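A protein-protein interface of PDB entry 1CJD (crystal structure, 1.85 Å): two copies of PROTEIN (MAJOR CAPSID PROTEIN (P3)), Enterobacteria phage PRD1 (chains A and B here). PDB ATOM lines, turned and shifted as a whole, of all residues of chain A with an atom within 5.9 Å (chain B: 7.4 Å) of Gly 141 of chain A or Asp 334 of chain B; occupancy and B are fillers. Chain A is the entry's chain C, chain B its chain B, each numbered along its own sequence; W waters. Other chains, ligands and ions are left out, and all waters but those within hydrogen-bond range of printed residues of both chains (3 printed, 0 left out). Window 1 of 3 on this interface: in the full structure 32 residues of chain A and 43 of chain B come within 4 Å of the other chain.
NH2 of Arg 328 of chain B is in salt-bridge range of OD2 of Asp 334 of chain B. OG of Ser 131 of chain A sits close to O of Gly 141 of chain A (3.3 Å). The side-chain amide oxygen of Asn 145 of chain A lies close to the side-chain carboxylate of Asp 142 of chain A, at 3.0 Å.
OH of Tyr 140 of chain A lies within hydrogen-bond range of OG1 of Thr 121 of chain B, 2.7 Å away. The side-chain amino group (NZ) of Lys 321 of chain B sits close to the backbone carbonyl oxygen (O) of Met 144 of chain A (3.4 Å). The side-chain amino group (NZ) of Lys 321 of chain B sits at hydrogen-bond distance from the backbone carbonyl oxygen (O) of Asn 145 of chain A (2.9 Å). The side-chain carboxylate (OD1) of Asp 142 of chain A is in salt-bridge range of the guanidinium group (NH2) of Arg 328 of chain B (3.1 Å). The backbone carbonyl oxygen of Ala 332 of chain B lies within hydrogen-bond range of the backbone NH of Met 132 of chain A (2.9 Å). The side-chain hydroxyl (OG1) of Thr 333 of chain B lies within hydrogen-bond range of the side-chain hydroxyl (OG) of Ser 131 of chain A (2.6 Å). OG1 of Thr 333 of chain B sits at hydrogen-bond distance from N of Gly 141 of chain A, 3.2 Å away. The backbone carbonyl oxygen of Gly 141 of chain A sits close to the backbone NH of Asp 334 of chain B (3.4 Å). N of Val 143 of chain A is in hydrogen-bond range of OD2 of Asp 334 of chain B (2.8 Å). N of Met 144 of chain A lies within hydrogen-bond range of OD2 of Asp 334 of chain B (2.8 Å).
No position is printed for both chains.
Ser 131 of chain A touches Ala 332 of chain B. Pro 336 of chain B touches Lys 139 of chain A (CA to O, 3.5 Å). Asp 334 of chain B touches Tyr 140 of chain A. Asp 142 of chain A touches Asp 334 of chain B (C to OD2, 3.7 Å). CG1 of Val 143 of chain A touches CG of Lys 337 of chain B, 3.7 Å away. NH2 of Arg 328 of chain B touches N of Asn 145 of chain A (3.6 Å). Lys 321 of chain B touches Val 146 of chain A. CG2 of Val 146 of chain A touches CB of Ala 324 of chain B (3.9 Å). Val 146 of chain A touches Ala 325 of chain B (CG1 to CB, 3.7 Å). CG2 of Val 146 of chain A touches NE of Arg 328 of chain B, 3.3 Å away.
Water W1 lies within hydrogen-bond range of the side-chain hydroxyl (OG1) of Thr 333 of chain B (2.8 Å) and the backbone carbonyl oxygen (O) of Met 132 of chain A (2.8 Å). Water W2 bridges the backbone carbonyl oxygen of Lys 139 of chain A (2.8 Å) and the backbone NH of Lys 337 of chain B (3.0 Å). Water W3 lies within hydrogen-bond range of the backbone carbonyl oxygen of Ala 332 of chain B and the backbone NH of Met 132 of chain A.
Of chain B, only Thr 333 and Asp 334 come within 4 Å of Gly 141 of chain A. Of the printed residues of chain A, Thr 121 of chain B touches Tyr 140. Printed residues of chain A within 4 Å of Lys 321 of chain B: Met 144 (3.2 Å), Asn 145 (2.9 Å) and Val 146 (3.9 Å). Trp 323 of chain B touches none of the printed residues of chain A. Of the printed residues of chain A, Ala 332 of chain B touches Ser 131 and Met 132. Asp 334 of chain B touches just these residues of chain A: Tyr 140, Gly 141, Asp 142, Val 143 and Met 144. The nearest printed residue of chain A that does not touch Lys 321 of chain B is Val 143 of chain A (7.1 Å).
Of the 16 printed residues of chain B, 12 touch a printed residue of chain A. Among the printed residues, Asp or Glu carboxylates within 4 Å of a Lys or Arg side-chain nitrogen of the other chain: Asp 142 of chain A with Arg 328 of chain B (3.1 Å).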
ATOM      1  N   SER A 131     -32.876 -16.401   2.193  1.00  0.00           N
ATOM      2  CA  SER A 131     -31.836 -17.202   1.590  1.00  0.00           C
ATOM      3  C   SER A 131     -32.353 -17.591   0.189  1.00  0.00           C
ATOM      4  O   SER A 131     -33.336 -18.313   0.048  1.00  0.00           O
ATOM      5  CB  SER A 131     -31.555 -18.459   2.406  1.00  0.00           C
ATOM      6  OG  SER A 131     -30.705 -19.330   1.671  1.00  0.00           O
ATOM      7  N   MET A 132     -31.669 -17.075  -0.833  1.00  0.00           N
ATOM      8  CA  MET A 132     -31.957 -17.299  -2.250  1.00  0.00           C
ATOM      9  C   MET A 132     -31.653 -18.761  -2.593  1.00  0.00           C
ATOM     10  O   MET A 132     -30.666 -19.301  -2.110  1.00  0.00           O
ATOM     11  CB  MET A 132     -31.037 -16.365  -3.048  1.00  0.00           C
ATOM     12  CG  MET A 132     -31.266 -16.294  -4.539  1.00  0.00           C
ATOM     13  SD  MET A 132     -29.817 -15.520  -5.398  1.00  0.00           S
ATOM     14  CE  MET A 132     -28.528 -15.968  -4.376  1.00  0.00           C
ATOM     15  N   LYS A 139     -22.924 -26.677  -0.005  1.00  0.00           N
ATOM     16  CA  LYS A 139     -24.100 -26.539   0.848  1.00  0.00           C
ATOM     17  C   LYS A 139     -24.467 -25.209   1.531  1.00  0.00           C
ATOM     18  O   LYS A 139     -24.614 -25.129   2.767  1.00  0.00           O
ATOM     19  CB  LYS A 139     -24.136 -27.713   1.845  1.00  0.00           C
ATOM     20  CG  LYS A 139     -24.039 -29.071   1.100  1.00  0.00           C
ATOM     21  CD  LYS A 139     -24.711 -30.226   1.811  1.00  0.00           C
ATOM     22  CE  LYS A 139     -24.613 -31.471   0.949  1.00  0.00           C
ATOM     23  NZ  LYS A 139     -24.843 -32.750   1.691  1.00  0.00           N
ATOM     24  N   TYR A 140     -24.616 -24.182   0.681  1.00  0.00           N
ATOM     25  CA  TYR A 140     -25.104 -22.849   1.070  1.00  0.00           C
ATOM     26  C   TYR A 140     -26.612 -23.136   1.152  1.00  0.00           C
ATOM     27  O   TYR A 140     -27.058 -24.173   0.660  1.00  0.00           O
ATOM     28  CB  TYR A 140     -24.936 -21.833  -0.072  1.00  0.00           C
ATOM     29  CG  TYR A 140     -23.522 -21.529  -0.434  1.00  0.00           C
ATOM     30  CD1 TYR A 140     -22.791 -20.615   0.306  1.00  0.00           C
ATOM     31  CD2 TYR A 140     -22.908 -22.142  -1.518  1.00  0.00           C
ATOM     32  CE1 TYR A 140     -21.471 -20.307  -0.018  1.00  0.00           C
ATOM     33  CE2 TYR A 140     -21.579 -21.839  -1.850  1.00  0.00           C
ATOM     34  CZ  TYR A 140     -20.875 -20.912  -1.084  1.00  0.00           C
ATOM     35  OH  TYR A 140     -19.581 -20.550  -1.393  1.00  0.00           O
ATOM     36  N   GLY A 141     -27.400 -22.228   1.714  1.00  0.00           N
ATOM     37  CA  GLY A 141     -28.826 -22.465   1.763  1.00  0.00           C
ATOM     38  C   GLY A 141     -29.381 -21.947   3.058  1.00  0.00           C
ATOM     39  O   GLY A 141     -28.757 -21.097   3.704  1.00  0.00           O
ATOM     40  N   ASP A 142     -30.561 -22.435   3.432  1.00  0.00           N
ATOM     41  CA  ASP A 142     -31.170 -22.029   4.693  1.00  0.00           C
ATOM     42  C   ASP A 142     -30.460 -22.897   5.730  1.00  0.00           C
ATOM     43  O   ASP A 142     -30.918 -23.974   6.065  1.00  0.00           O
ATOM     44  CB  ASP A 142     -32.678 -22.319   4.665  1.00  0.00           C
ATOM     45  CG  ASP A 142     -33.366 -21.987   5.972  1.00  0.00           C
ATOM     46  OD1 ASP A 142     -32.674 -21.435   6.860  1.00  0.00           O
ATOM     47  OD2 ASP A 142     -34.595 -22.277   6.103  1.00  0.00           O
ATOM     48  N   VAL A 143     -29.329 -22.420   6.222  1.00  0.00           N
ATOM     49  CA  VAL A 143     -28.532 -23.174   7.180  1.00  0.00           C
ATOM     50  C   VAL A 143     -28.841 -22.722   8.587  1.00  0.00           C
ATOM     51  O   VAL A 143     -28.984 -23.542   9.504  1.00  0.00           O
ATOM     52  CB  VAL A 143     -26.964 -22.936   6.946  1.00  0.00           C
ATOM     53  CG1 VAL A 143     -26.125 -23.561   8.085  1.00  0.00           C
ATOM     54  CG2 VAL A 143     -26.543 -23.472   5.606  1.00  0.00           C
ATOM     55  N   MET A 144     -28.956 -21.405   8.736  1.00  0.00           N
ATOM     56  CA  MET A 144     -29.113 -20.783  10.035  1.00  0.00           C
ATOM     57  C   MET A 144     -30.498 -20.342  10.441  1.00  0.00           C
ATOM     58  O   MET A 144     -30.685 -19.845  11.549  1.00  0.00           O
ATOM     59  CB  MET A 144     -28.144 -19.602  10.125  1.00  0.00           C
ATOM     60  CG  MET A 144     -26.668 -20.008  10.135  1.00  0.00           C
ATOM     61  SD  MET A 144     -26.260 -20.862  11.668  1.00  0.00           S
ATOM     62  CE  MET A 144     -26.709 -19.616  12.942  1.00  0.00           C
ATOM     63  N   ASN A 145     -31.456 -20.523   9.544  1.00  0.00           N
ATOM     64  CA  ASN A 145     -32.839 -20.158   9.812  1.00  0.00           C
ATOM     65  C   ASN A 145     -33.046 -18.774  10.415  1.00  0.00           C
ATOM     66  O   ASN A 145     -33.747 -18.623  11.417  1.00  0.00           O
ATOM     67  CB  ASN A 145     -33.443 -21.221  10.715  1.00  0.00           C
ATOM     68  CG  ASN A 145     -33.743 -22.476   9.953  1.00  0.00           C
ATOM     69  OD1 ASN A 145     -34.622 -22.501   9.064  1.00  0.00           O
ATOM     70  ND2 ASN A 145     -33.009 -23.517  10.262  1.00  0.00           N
ATOM     71  N   VAL A 146     -32.447 -17.771   9.785  1.00  0.00           N
ATOM     72  CA  VAL A 146     -32.528 -16.389  10.255  1.00  0.00           C
ATOM     73  C   VAL A 146     -33.963 -15.877  10.349  1.00  0.00           C
ATOM     74  O   VAL A 146     -34.330 -15.305  11.370  1.00  0.00           O
ATOM     75  CB  VAL A 146     -31.654 -15.497   9.371  1.00  0.00           C
ATOM     76  CG1 VAL A 146     -31.718 -14.027   9.851  1.00  0.00           C
ATOM     77  CG2 VAL A 146     -30.214 -16.047   9.437  1.00  0.00           C
ATOM     78  N   THR B 121     -17.233 -16.374  -3.440  1.00  0.00           N
ATOM     79  CA  THR B 121     -18.649 -16.167  -3.147  1.00  0.00           C
ATOM     80  C   THR B 121     -18.890 -14.792  -2.498  1.00  0.00           C
ATOM     81  O   THR B 121     -19.772 -14.013  -2.918  1.00  0.00           O
ATOM     82  CB  THR B 121     -19.178 -17.287  -2.236  1.00  0.00           C
ATOM     83  OG1 THR B 121     -19.373 -18.465  -3.028  1.00  0.00           O
ATOM     84  CG2 THR B 121     -20.517 -16.900  -1.587  1.00  0.00           C
ATOM     85  N   PRO B 127     -23.542 -17.255  -4.031  1.00  0.00           N
ATOM     86  CA  PRO B 127     -22.709 -18.458  -4.250  1.00  0.00           C
ATOM     87  C   PRO B 127     -22.011 -18.353  -5.621  1.00  0.00           C
ATOM     88  O   PRO B 127     -22.663 -18.223  -6.675  1.00  0.00           O
ATOM     89  CB  PRO B 127     -23.716 -19.600  -4.175  1.00  0.00           C
ATOM     90  CG  PRO B 127     -24.712 -19.077  -3.147  1.00  0.00           C
ATOM     91  CD  PRO B 127     -24.869 -17.606  -3.500  1.00  0.00           C
ATOM     92  N   LYS B 321     -27.245 -16.485  15.188  1.00  0.00           N
ATOM     93  CA  LYS B 321     -28.272 -16.157  14.193  1.00  0.00           C
ATOM     94  C   LYS B 321     -28.156 -14.729  13.684  1.00  0.00           C
ATOM     95  O   LYS B 321     -28.317 -14.483  12.499  1.00  0.00           O
ATOM     96  CB  LYS B 321     -29.670 -16.374  14.767  1.00  0.00           C
ATOM     97  CG  LYS B 321     -30.644 -16.999  13.787  1.00  0.00           C
ATOM     98  CD  LYS B 321     -31.845 -17.628  14.505  1.00  0.00           C
ATOM     99  CE  LYS B 321     -31.766 -19.156  14.492  1.00  0.00           C
ATOM    100  NZ  LYS B 321     -33.026 -19.793  13.986  1.00  0.00           N
ATOM    101  N   TRP B 323     -25.415 -12.973  13.706  1.00  0.00           N
ATOM    102  CA  TRP B 323     -24.177 -12.902  12.945  1.00  0.00           C
ATOM    103  C   TRP B 323     -24.504 -13.405  11.510  1.00  0.00           C
ATOM    104  O   TRP B 323     -24.119 -12.802  10.493  1.00  0.00           O
ATOM    105  CB  TRP B 323     -23.130 -13.796  13.609  1.00  0.00           C
ATOM    106  CG  TRP B 323     -21.783 -13.731  12.938  1.00  0.00           C
ATOM    107  CD1 TRP B 323     -21.398 -14.387  11.801  1.00  0.00           C
ATOM    108  CD2 TRP B 323     -20.650 -12.983  13.374  1.00  0.00           C
ATOM    109  NE1 TRP B 323     -20.097 -14.090  11.503  1.00  0.00           N
ATOM    110  CE2 TRP B 323     -19.610 -13.230  12.453  1.00  0.00           C
ATOM    111  CE3 TRP B 323     -20.409 -12.125  14.452  1.00  0.00           C
ATOM    112  CZ2 TRP B 323     -18.340 -12.648  12.582  1.00  0.00           C
ATOM    113  CZ3 TRP B 323     -19.150 -11.541  14.578  1.00  0.00           C
ATOM    114  CH2 TRP B 323     -18.133 -11.809  13.647  1.00  0.00           C
ATOM    115  N   ALA B 324     -25.241 -14.504  11.432  1.00  0.00           N
ATOM    116  CA  ALA B 324     -25.626 -15.054  10.146  1.00  0.00           C
ATOM    117  C   ALA B 324     -26.496 -14.043   9.344  1.00  0.00           C
ATOM    118  O   ALA B 324     -26.416 -13.979   8.104  1.00  0.00           O
ATOM    119  CB  ALA B 324     -26.398 -16.364  10.363  1.00  0.00           C
ATOM    120  N   ALA B 325     -27.340 -13.275  10.047  1.00  0.00           N
ATOM    121  CA  ALA B 325     -28.202 -12.288   9.410  1.00  0.00           C
ATOM    122  C   ALA B 325     -27.316 -11.279   8.677  1.00  0.00           C
ATOM    123  O   ALA B 325     -27.604 -10.894   7.533  1.00  0.00           O
ATOM    124  CB  ALA B 325     -29.063 -11.590  10.453  1.00  0.00           C
ATOM    125  N   THR B 327     -24.426 -11.810   7.383  1.00  0.00           N
ATOM    126  CA  THR B 327     -23.888 -12.496   6.221  1.00  0.00           C
ATOM    127  C   THR B 327     -24.945 -12.649   5.124  1.00  0.00           C
ATOM    128  O   THR B 327     -24.624 -12.549   3.939  1.00  0.00           O
ATOM    129  CB  THR B 327     -23.308 -13.856   6.641  1.00  0.00           C
ATOM    130  OG1 THR B 327     -22.107 -13.621   7.386  1.00  0.00           O
ATOM    131  CG2 THR B 327     -22.982 -14.721   5.441  1.00  0.00           C
ATOM    132  N   ARG B 328     -26.201 -12.882   5.511  1.00  0.00           N
ATOM    133  CA  ARG B 328     -27.277 -13.002   4.515  1.00  0.00           C
ATOM    134  C   ARG B 328     -27.395 -11.703   3.686  1.00  0.00           C
ATOM    135  O   ARG B 328     -27.829 -11.734   2.525  1.00  0.00           O
ATOM    136  CB  ARG B 328     -28.609 -13.305   5.206  1.00  0.00           C
ATOM    137  CG  ARG B 328     -28.727 -14.756   5.619  1.00  0.00           C
ATOM    138  CD  ARG B 328     -30.183 -15.177   5.779  1.00  0.00           C
ATOM    139  NE  ARG B 328     -30.270 -16.589   6.150  1.00  0.00           N
ATOM    140  CZ  ARG B 328     -31.400 -17.302   6.147  1.00  0.00           C
ATOM    141  NH1 ARG B 328     -32.556 -16.732   5.789  1.00  0.00           N
ATOM    142  NH2 ARG B 328     -31.365 -18.601   6.474  1.00  0.00           N
ATOM    143  N   ILE B 331     -24.143 -12.180   1.021  1.00  0.00           N
ATOM    144  CA  ILE B 331     -24.141 -13.208  -0.016  1.00  0.00           C
ATOM    145  C   ILE B 331     -25.513 -13.778  -0.333  1.00  0.00           C
ATOM    146  O   ILE B 331     -25.611 -14.763  -1.062  1.00  0.00           O
ATOM    147  CB  ILE B 331     -23.140 -14.358   0.325  1.00  0.00           C
ATOM    148  CG1 ILE B 331     -23.564 -15.103   1.593  1.00  0.00           C
ATOM    149  CG2 ILE B 331     -21.758 -13.777   0.536  1.00  0.00           C
ATOM    150  CD1 ILE B 331     -23.037 -16.522   1.667  1.00  0.00           C
ATOM    151  N   ALA B 332     -26.559 -13.142   0.213  1.00  0.00           N
ATOM    152  CA  ALA B 332     -27.947 -13.498  -0.041  1.00  0.00           C
ATOM    153  C   ALA B 332     -28.380 -14.880   0.432  1.00  0.00           C
ATOM    154  O   ALA B 332     -29.434 -15.368   0.015  1.00  0.00           O
ATOM    155  CB  ALA B 332     -28.241 -13.348  -1.559  1.00  0.00           C
ATOM    156  N   THR B 333     -27.587 -15.496   1.306  1.00  0.00           N
ATOM    157  CA  THR B 333     -27.863 -16.839   1.821  1.00  0.00           C
ATOM    158  C   THR B 333     -26.864 -17.085   2.968  1.00  0.00           C
ATOM    159  O   THR B 333     -26.124 -16.176   3.352  1.00  0.00           O
ATOM    160  CB  THR B 333     -27.668 -17.905   0.684  1.00  0.00           C
ATOM    161  OG1 THR B 333     -28.136 -19.192   1.127  1.00  0.00           O
ATOM    162  CG2 THR B 333     -26.197 -18.005   0.260  1.00  0.00           C
ATOM    163  N   ASP B 334     -26.864 -18.290   3.534  1.00  0.00           N
ATOM    164  CA  ASP B 334     -25.910 -18.622   4.604  1.00  0.00           C
ATOM    165  C   ASP B 334     -24.728 -19.420   4.024  1.00  0.00           C
ATOM    166  O   ASP B 334     -24.896 -20.146   3.041  1.00  0.00           O
ATOM    167  CB  ASP B 334     -26.555 -19.550   5.656  1.00  0.00           C
ATOM    168  CG  ASP B 334     -27.762 -18.935   6.337  1.00  0.00           C
ATOM    169  OD1 ASP B 334     -27.696 -17.732   6.656  1.00  0.00           O
ATOM    170  OD2 ASP B 334     -28.756 -19.670   6.558  1.00  0.00           O
ATOM    171  N   PHE B 335     -23.547 -19.302   4.630  1.00  0.00           N
ATOM    172  CA  PHE B 335     -22.406 -20.139   4.228  1.00  0.00           C
ATOM    173  C   PHE B 335     -22.723 -21.510   4.873  1.00  0.00           C
ATOM    174  O   PHE B 335     -23.600 -21.589   5.751  1.00  0.00           O
ATOM    175  CB  PHE B 335     -21.117 -19.604   4.835  1.00  0.00           C
ATOM    176  CG  PHE B 335     -20.427 -18.584   3.977  1.00  0.00           C
ATOM    177  CD1 PHE B 335     -19.748 -18.971   2.832  1.00  0.00           C
ATOM    178  CD2 PHE B 335     -20.474 -17.236   4.318  1.00  0.00           C
ATOM    179  CE1 PHE B 335     -19.113 -18.037   2.019  1.00  0.00           C
ATOM    180  CE2 PHE B 335     -19.843 -16.286   3.510  1.00  0.00           C
ATOM    181  CZ  PHE B 335     -19.158 -16.695   2.349  1.00  0.00           C
ATOM    182  N   PRO B 336     -22.024 -22.599   4.464  1.00  0.00           N
ATOM    183  CA  PRO B 336     -22.327 -23.907   5.075  1.00  0.00           C
ATOM    184  C   PRO B 336     -22.207 -23.975   6.616  1.00  0.00           C
ATOM    185  O   PRO B 336     -21.650 -23.086   7.273  1.00  0.00           O
ATOM    186  CB  PRO B 336     -21.359 -24.876   4.366  1.00  0.00           C
ATOM    187  CG  PRO B 336     -21.007 -24.183   3.058  1.00  0.00           C
ATOM    188  CD  PRO B 336     -20.976 -22.707   3.426  1.00  0.00           C
ATOM    189  N   LYS B 337     -22.747 -25.047   7.178  1.00  0.00           N
ATOM    190  CA  LYS B 337     -22.732 -25.245   8.622  1.00  0.00           C
ATOM    191  C   LYS B 337     -21.349 -25.023   9.245  1.00  0.00           C
ATOM    192  O   LYS B 337     -20.332 -25.590   8.777  1.00  0.00           O
ATOM    193  CB  LYS B 337     -23.197 -26.668   8.937  1.00  0.00           C
ATOM    194  CG  LYS B 337     -24.658 -26.893   8.749  1.00  0.00           C
ATOM    195  CD  LYS B 337     -25.068 -28.215   9.360  1.00  0.00           C
ATOM    196  CE  LYS B 337     -24.665 -29.367   8.473  1.00  0.00           C
ATOM    197  NZ  LYS B 337     -24.049 -30.453   9.261  1.00  0.00           N
ATOM    198  N   VAL B 339     -19.509 -22.412   9.170  1.00  0.00           N
ATOM    199  CA  VAL B 339     -18.664 -21.440   8.463  1.00  0.00           C
ATOM    200  C   VAL B 339     -19.218 -20.050   8.764  1.00  0.00           C
ATOM    201  O   VAL B 339     -20.384 -19.792   8.483  1.00  0.00           O
ATOM    202  CB  VAL B 339     -18.689 -21.667   6.932  1.00  0.00           C
ATOM    203  CG1 VAL B 339     -17.786 -20.646   6.241  1.00  0.00           C
ATOM    204  CG2 VAL B 339     -18.229 -23.085   6.596  1.00  0.00           C
HETATM  205  O   HOH W   1     -28.386 -20.581  -1.235  1.00  0.00           O
HETATM  206  O   HOH W   2     -24.259 -26.582   5.132  1.00  0.00           O
HETATM  207  O   HOH W   3     -31.917 -13.656  -0.752  1.00  0.00           O
